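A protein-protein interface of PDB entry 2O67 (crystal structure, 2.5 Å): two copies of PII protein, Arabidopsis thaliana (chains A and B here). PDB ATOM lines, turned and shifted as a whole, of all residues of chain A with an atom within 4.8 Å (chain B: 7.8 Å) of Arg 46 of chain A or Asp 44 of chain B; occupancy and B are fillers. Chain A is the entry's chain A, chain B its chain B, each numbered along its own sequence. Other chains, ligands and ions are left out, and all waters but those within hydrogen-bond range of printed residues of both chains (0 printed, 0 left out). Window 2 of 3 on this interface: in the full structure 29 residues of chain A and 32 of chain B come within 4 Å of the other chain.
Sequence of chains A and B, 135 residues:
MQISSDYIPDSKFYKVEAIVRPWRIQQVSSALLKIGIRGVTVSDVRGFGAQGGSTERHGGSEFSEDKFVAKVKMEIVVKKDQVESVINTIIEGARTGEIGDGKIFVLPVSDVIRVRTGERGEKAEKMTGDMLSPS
Hydrophobic or aromatic side chains of chain B that line the printed part of chain A: Val 42. Of the 7 printed residues of chain A, 5 touch a printed residue of chain B. Among the printed residues, 9 pairs touch across the chains.
N of Glu 75 of chain B sits at hydrogen-bond distance from O of Thr 41 of chain B, at 2.6 Å. N of Val 69 of chain A lies within hydrogen-bond range of O of Gly 47 of chain A (2.7 Å). O of Ser 43 of chain B is in hydrogen-bond range of N of Lys 73 of chain B.
Arg 46 of chain A touches Asp 44 of chain B, but with the chains exchanged Asp 44 of chain A does not touch Arg 46 of chain B (10.3 Å). 3 positions are printed for both chains. Of the 9 pairs that touch across the chains among the printed residues, none has its exchanged pair printed and touching as well.
Printed residues of chain B within 4 Å of Asp 44 of chain A: Ser 43. Arg 46 of chain A touches just these residues of chain B: Thr 41 (3.7 Å), Val 42 (2.8 Å) and Asp 44 (3.1 Å). Of the printed residues of chain A, Val 40 of chain B touches Gly 47 (3.9 Å) and Phe 48 (3.5 Å). Asp 44 of chain B touches one residue of chain A. The nearest residue of chain B that does not touch Arg 46 of chain A is Val 40 of chain B (4.1 Å).
Among the printed residues, pairs that only touch across the chains: Asp 44 of chain A with Ser 43 of chain B (3.8 Å), Val 45 of chain A with Thr 41 of chain B (3.8 Å), Val 45 of chain A with Val 42 of chain B (3.5 Å), Arg 46 of chain A with Thr 41 of chain B (3.7 Å), Gly 47 of chain A with Val 40 of chain B (3.9 Å) and Phe 48 of chain A with Val 42 of chain B (3.7 Å).
The backbone NH (N) of Phe 48 of chain A sits at hydrogen-bond distance from the backbone carbonyl oxygen (O) of Val 40 of chain B (3.5 Å). NH1 of Arg 46 of chain A is in salt-bridge range of OD2 of Asp 44 of chain B, at 3.1 Å. The backbone carbonyl oxygen (O) of Val 42 of chain B lies within hydrogen-bond range of the backbone NH (N) of Arg 46 of chain A.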
ATOM      1  N   ASP A  44      25.542 -22.803  15.263  1.00  0.00           N
ATOM      2  CA  ASP A  44      24.299 -22.273  15.800  1.00  0.00           C
ATOM      3  C   ASP A  44      23.159 -23.235  15.560  1.00  0.00           C
ATOM      4  O   ASP A  44      22.975 -23.734  14.452  1.00  0.00           O
ATOM      5  CB  ASP A  44      23.976 -20.924  15.174  1.00  0.00           C
ATOM      6  CG  ASP A  44      25.017 -19.883  15.487  1.00  0.00           C
ATOM      7  OD1 ASP A  44      25.309 -19.676  16.686  1.00  0.00           O
ATOM      8  OD2 ASP A  44      25.546 -19.276  14.533  1.00  0.00           O
ATOM      9  N   VAL A  45      22.413 -23.512  16.621  1.00  0.00           N
ATOM     10  CA  VAL A  45      21.213 -24.336  16.534  1.00  0.00           C
ATOM     11  C   VAL A  45      20.029 -23.567  17.123  1.00  0.00           C
ATOM     12  O   VAL A  45      20.204 -22.587  17.852  1.00  0.00           O
ATOM     13  CB  VAL A  45      21.389 -25.735  17.209  1.00  0.00           C
ATOM     14  CG1 VAL A  45      22.464 -26.545  16.495  1.00  0.00           C
ATOM     15  CG2 VAL A  45      21.721 -25.611  18.684  1.00  0.00           C
ATOM     16  N   ARG A  46      18.824 -23.990  16.773  1.00  0.00           N
ATOM     17  CA  ARG A  46      17.620 -23.369  17.297  1.00  0.00           C
ATOM     18  C   ARG A  46      16.768 -24.446  17.947  1.00  0.00           C
ATOM     19  O   ARG A  46      16.504 -25.496  17.351  1.00  0.00           O
ATOM     20  CB  ARG A  46      16.848 -22.635  16.195  1.00  0.00           C
ATOM     21  CG  ARG A  46      17.647 -21.520  15.518  1.00  0.00           C
ATOM     22  CD  ARG A  46      16.863 -20.827  14.403  1.00  0.00           C
ATOM     23  NE  ARG A  46      16.267 -21.763  13.443  1.00  0.00           N
ATOM     24  CZ  ARG A  46      16.912 -22.324  12.420  1.00  0.00           C
ATOM     25  NH1 ARG A  46      18.202 -22.073  12.204  1.00  0.00           N
ATOM     26  NH2 ARG A  46      16.262 -23.152  11.614  1.00  0.00           N
ATOM     27  N   GLY A  47      16.377 -24.194  19.188  1.00  0.00           N
ATOM     28  CA  GLY A  47      15.519 -25.106  19.914  1.00  0.00           C
ATOM     29  C   GLY A  47      14.082 -24.641  19.850  1.00  0.00           C
ATOM     30  O   GLY A  47      13.745 -23.558  20.311  1.00  0.00           O
ATOM     31  N   PHE A  48      13.241 -25.455  19.233  1.00  0.00           N
ATOM     32  CA  PHE A  48      11.800 -25.287  19.330  1.00  0.00           C
ATOM     33  C   PHE A  48      11.380 -26.258  20.419  1.00  0.00           C
ATOM     34  O   PHE A  48      10.210 -26.336  20.810  1.00  0.00           O
ATOM     35  CB  PHE A  48      11.140 -25.540  17.972  1.00  0.00           C
ATOM     36  CG  PHE A  48      11.555 -24.539  16.918  1.00  0.00           C
ATOM     37  CD1 PHE A  48      12.775 -24.668  16.251  1.00  0.00           C
ATOM     38  CD2 PHE A  48      10.749 -23.445  16.621  1.00  0.00           C
ATOM     39  CE1 PHE A  48      13.176 -23.733  15.290  1.00  0.00           C
ATOM     40  CE2 PHE A  48      11.141 -22.498  15.660  1.00  0.00           C
ATOM     41  CZ  PHE A  48      12.354 -22.647  14.991  1.00  0.00           C
ATOM     42  N   PHE A  68      11.662 -19.734  18.983  1.00  0.00           N
ATOM     43  CA  PHE A  68      12.748 -20.651  19.343  1.00  0.00           C
ATOM     44  C   PHE A  68      13.709 -20.104  20.394  1.00  0.00           C
ATOM     45  O   PHE A  68      13.767 -18.897  20.641  1.00  0.00           O
ATOM     46  CB  PHE A  68      13.545 -21.073  18.098  1.00  0.00           C
ATOM     47  CG  PHE A  68      14.360 -19.966  17.481  1.00  0.00           C
ATOM     48  CD1 PHE A  68      15.637 -19.672  17.955  1.00  0.00           C
ATOM     49  CD2 PHE A  68      13.859 -19.228  16.416  1.00  0.00           C
ATOM     50  CE1 PHE A  68      16.397 -18.648  17.388  1.00  0.00           C
ATOM     51  CE2 PHE A  68      14.614 -18.204  15.838  1.00  0.00           C
ATOM     52  CZ  PHE A  68      15.883 -17.914  16.322  1.00  0.00           C
ATOM     53  N   VAL A  69      14.465 -21.012  21.007  1.00  0.00           N
ATOM     54  CA  VAL A  69      15.582 -20.642  21.867  1.00  0.00           C
ATOM     55  C   VAL A  69      16.906 -20.867  21.129  1.00  0.00           C
ATOM     56  O   VAL A  69      17.149 -21.953  20.597  1.00  0.00           O
ATOM     57  CB  VAL A  69      15.533 -21.380  23.257  1.00  0.00           C
ATOM     58  CG1 VAL A  69      14.985 -22.796  23.123  1.00  0.00           C
ATOM     59  CG2 VAL A  69      16.901 -21.382  23.950  1.00  0.00           C
ATOM     60  N   PRO B  22      12.712 -26.565   4.832  1.00  0.00           N
ATOM     61  CA  PRO B  22      12.721 -25.544   5.887  1.00  0.00           C
ATOM     62  C   PRO B  22      11.341 -25.137   6.401  1.00  0.00           C
ATOM     63  O   PRO B  22      11.217 -24.701   7.551  1.00  0.00           O
ATOM     64  CB  PRO B  22      13.406 -24.343   5.217  1.00  0.00           C
ATOM     65  CG  PRO B  22      14.148 -24.911   4.059  1.00  0.00           C
ATOM     66  CD  PRO B  22      13.327 -26.065   3.588  1.00  0.00           C
ATOM     67  N   ILE B  25       9.197 -27.408   9.559  1.00  0.00           N
ATOM     68  CA  ILE B  25       9.585 -27.429  10.977  1.00  0.00           C
ATOM     69  C   ILE B  25       8.373 -27.596  11.887  1.00  0.00           C
ATOM     70  O   ILE B  25       8.298 -28.554  12.661  1.00  0.00           O
ATOM     71  CB  ILE B  25      10.387 -26.161  11.413  1.00  0.00           C
ATOM     72  CG1 ILE B  25      11.642 -25.967  10.559  1.00  0.00           C
ATOM     73  CG2 ILE B  25      10.780 -26.248  12.900  1.00  0.00           C
ATOM     74  CD1 ILE B  25      12.304 -24.601  10.731  1.00  0.00           C
ATOM     75  N   GLY B  39      11.469 -31.740  22.662  1.00  0.00           N
ATOM     76  CA  GLY B  39      12.717 -31.020  22.425  1.00  0.00           C
ATOM     77  C   GLY B  39      13.509 -31.359  21.176  1.00  0.00           C
ATOM     78  O   GLY B  39      14.541 -32.036  21.253  1.00  0.00           O
ATOM     79  N   VAL B  40      13.042 -30.865  20.032  1.00  0.00           N
ATOM     80  CA  VAL B  40      13.787 -30.991  18.776  1.00  0.00           C
ATOM     81  C   VAL B  40      14.768 -29.824  18.579  1.00  0.00           C
ATOM     82  O   VAL B  40      14.458 -28.674  18.900  1.00  0.00           O
ATOM     83  CB  VAL B  40      12.840 -31.175  17.543  1.00  0.00           C
ATOM     84  CG1 VAL B  40      12.120 -29.879  17.183  1.00  0.00           C
ATOM     85  CG2 VAL B  40      13.610 -31.717  16.347  1.00  0.00           C
ATOM     86  N   THR B  41      15.951 -30.150  18.061  1.00  0.00           N
ATOM     87  CA  THR B  41      17.006 -29.182  17.744  1.00  0.00           C
ATOM     88  C   THR B  41      17.104 -29.020  16.222  1.00  0.00           C
ATOM     89  O   THR B  41      17.123 -30.010  15.491  1.00  0.00           O
ATOM     90  CB  THR B  41      18.365 -29.644  18.360  1.00  0.00           C
ATOM     91  OG1 THR B  41      18.412 -29.261  19.737  1.00  0.00           O
ATOM     92  CG2 THR B  41      19.558 -29.036  17.648  1.00  0.00           C
ATOM     93  N   VAL B  42      17.176 -27.775  15.756  1.00  0.00           N
ATOM     94  CA  VAL B  42      17.118 -27.459  14.322  1.00  0.00           C
ATOM     95  C   VAL B  42      18.306 -26.610  13.862  1.00  0.00           C
ATOM     96  O   VAL B  42      18.700 -25.671  14.549  1.00  0.00           O
ATOM     97  CB  VAL B  42      15.807 -26.693  13.975  1.00  0.00           C
ATOM     98  CG1 VAL B  42      15.655 -26.535  12.468  1.00  0.00           C
ATOM     99  CG2 VAL B  42      14.582 -27.401  14.566  1.00  0.00           C
ATOM    100  N   SER B  43      18.862 -26.926  12.692  1.00  0.00           N
ATOM    101  CA  SER B  43      19.918 -26.094  12.092  1.00  0.00           C
ATOM    102  C   SER B  43      19.831 -25.991  10.575  1.00  0.00           C
ATOM    103  O   SER B  43      19.247 -26.845   9.917  1.00  0.00           O
ATOM    104  CB  SER B  43      21.320 -26.563  12.515  1.00  0.00           C
ATOM    105  OG  SER B  43      21.398 -27.976  12.596  1.00  0.00           O
ATOM    106  N   ASP B  44      20.429 -24.935  10.032  1.00  0.00           N
ATOM    107  CA  ASP B  44      20.454 -24.696   8.594  1.00  0.00           C
ATOM    108  C   ASP B  44      21.530 -25.519   7.919  1.00  0.00           C
ATOM    109  O   ASP B  44      22.697 -25.495   8.328  1.00  0.00           O
ATOM    110  CB  ASP B  44      20.673 -23.212   8.297  1.00  0.00           C
ATOM    111  CG  ASP B  44      19.541 -22.344   8.824  1.00  0.00           C
ATOM    112  OD1 ASP B  44      18.383 -22.551   8.409  1.00  0.00           O
ATOM    113  OD2 ASP B  44      19.809 -21.457   9.661  1.00  0.00           O
ATOM    114  N   VAL B  45      21.117 -26.255   6.891  1.00  0.00           N
ATOM    115  CA  VAL B  45      22.027 -27.030   6.054  1.00  0.00           C
ATOM    116  C   VAL B  45      21.709 -26.796   4.574  1.00  0.00           C
ATOM    117  O   VAL B  45      20.586 -26.419   4.219  1.00  0.00           O
ATOM    118  CB  VAL B  45      21.991 -28.547   6.386  1.00  0.00           C
ATOM    119  CG1 VAL B  45      22.438 -28.789   7.824  1.00  0.00           C
ATOM    120  CG2 VAL B  45      20.611 -29.122   6.154  1.00  0.00           C
ATOM    121  N   ARG B  46      22.708 -27.009   3.721  1.00  0.00           N
ATOM    122  CA  ARG B  46      22.565 -26.785   2.290  1.00  0.00           C
ATOM    123  C   ARG B  46      22.868 -28.059   1.504  1.00  0.00           C
ATOM    124  O   ARG B  46      23.840 -28.754   1.789  1.00  0.00           O
ATOM    125  CB  ARG B  46      23.477 -25.641   1.830  1.00  0.00           C
ATOM    126  CG  ARG B  46      23.176 -24.301   2.485  1.00  0.00           C
ATOM    127  CD  ARG B  46      24.086 -23.178   1.979  1.00  0.00           C
ATOM    128  NE  ARG B  46      25.515 -23.402   2.232  1.00  0.00           N
ATOM    129  CZ  ARG B  46      26.126 -23.219   3.405  1.00  0.00           C
ATOM    130  NH1 ARG B  46      25.443 -22.823   4.472  1.00  0.00           N
ATOM    131  NH2 ARG B  46      27.431 -23.441   3.513  1.00  0.00           N
ATOM    132  N   ALA B  70      18.280 -25.132   0.125  1.00  0.00           N
ATOM    133  CA  ALA B  70      18.135 -24.909   1.558  1.00  0.00           C
ATOM    134  C   ALA B  70      17.333 -26.035   2.205  1.00  0.00           C
ATOM    135  O   ALA B  70      16.250 -26.380   1.734  1.00  0.00           O
ATOM    136  CB  ALA B  70      17.486 -23.562   1.828  1.00  0.00           C
ATOM    137  N   LYS B  71      17.892 -26.614   3.267  1.00  0.00           N
ATOM    138  CA  LYS B  71      17.217 -27.627   4.081  1.00  0.00           C
ATOM    139  C   LYS B  71      17.477 -27.361   5.568  1.00  0.00           C
ATOM    140  O   LYS B  71      18.332 -26.550   5.928  1.00  0.00           O
ATOM    141  CB  LYS B  71      17.691 -29.042   3.715  1.00  0.00           C
ATOM    142  CG  LYS B  71      17.475 -29.444   2.254  1.00  0.00           C
ATOM    143  CD  LYS B  71      17.933 -30.876   1.987  1.00  0.00           C
ATOM    144  CE  LYS B  71      18.176 -31.141   0.499  1.00  0.00           C
ATOM    145  NZ  LYS B  71      16.910 -31.159  -0.302  1.00  0.00           N
ATOM    146  N   VAL B  72      16.736 -28.043   6.432  1.00  0.00           N
ATOM    147  CA  VAL B  72      16.996 -27.960   7.865  1.00  0.00           C
ATOM    148  C   VAL B  72      17.241 -29.344   8.455  1.00  0.00           C
ATOM    149  O   VAL B  72      16.492 -30.288   8.193  1.00  0.00           O
ATOM    150  CB  VAL B  72      15.869 -27.207   8.654  1.00  0.00           C
ATOM    151  CG1 VAL B  72      15.877 -25.721   8.327  1.00  0.00           C
ATOM    152  CG2 VAL B  72      14.492 -27.802   8.376  1.00  0.00           C
ATOM    153  N   LYS B  73      18.314 -29.454   9.235  1.00  0.00           N
ATOM    154  CA  LYS B  73      18.579 -30.649  10.022  1.00  0.00           C
ATOM    155  C   LYS B  73      17.807 -30.576  11.338  1.00  0.00           C
ATOM    156  O   LYS B  73      17.959 -29.626  12.089  1.00  0.00           O
ATOM    157  CB  LYS B  73      20.075 -30.788  10.297  1.00  0.00           C
ATOM    158  CG  LYS B  73      20.460 -32.137  10.906  1.00  0.00           C
ATOM    159  CD  LYS B  73      21.855 -32.114  11.496  1.00  0.00           C
ATOM    160  CE  LYS B  73      22.930 -32.006  10.432  1.00  0.00           C
ATOM    161  NZ  LYS B  73      24.189 -31.477  11.023  1.00  0.00           N
ATOM    162  N   MET B  74      16.970 -31.576  11.595  1.00  0.00           N
ATOM    163  CA  MET B  74      16.246 -31.686  12.858  1.00  0.00           C
ATOM    164  C   MET B  74      16.802 -32.859  13.656  1.00  0.00           C
ATOM    165  O   MET B  74      16.801 -34.002  13.188  1.00  0.00           O
ATOM    166  CB  MET B  74      14.744 -31.857  12.627  1.00  0.00           C
ATOM    167  CG  MET B  74      14.101 -30.719  11.839  1.00  0.00           C
ATOM    168  SD  MET B  74      12.306 -30.864  11.661  1.00  0.00           S
ATOM    169  CE  MET B  74      12.034 -29.636  10.401  1.00  0.00           C
ATOM    170  N   GLU B  75      17.276 -32.570  14.864  1.00  0.00           N
ATOM    171  CA  GLU B  75      17.950 -33.574  15.676  1.00  0.00           C
ATOM    172  C   GLU B  75      17.184 -33.899  16.942  1.00  0.00           C
ATOM    173  O   GLU B  75      16.775 -33.007  17.685  1.00  0.00           O
ATOM    174  CB  GLU B  75      19.357 -33.106  16.031  1.00  0.00           C
ATOM    175  CG  GLU B  75      20.243 -32.892  14.832  1.00  0.00           C
ATOM    176  CD  GLU B  75      21.396 -31.975  15.136  1.00  0.00           C
ATOM    177  OE1 GLU B  75      22.468 -32.484  15.516  1.00  0.00           O
ATOM    178  OE2 GLU B  75      21.224 -30.743  15.011  1.00  0.00           O
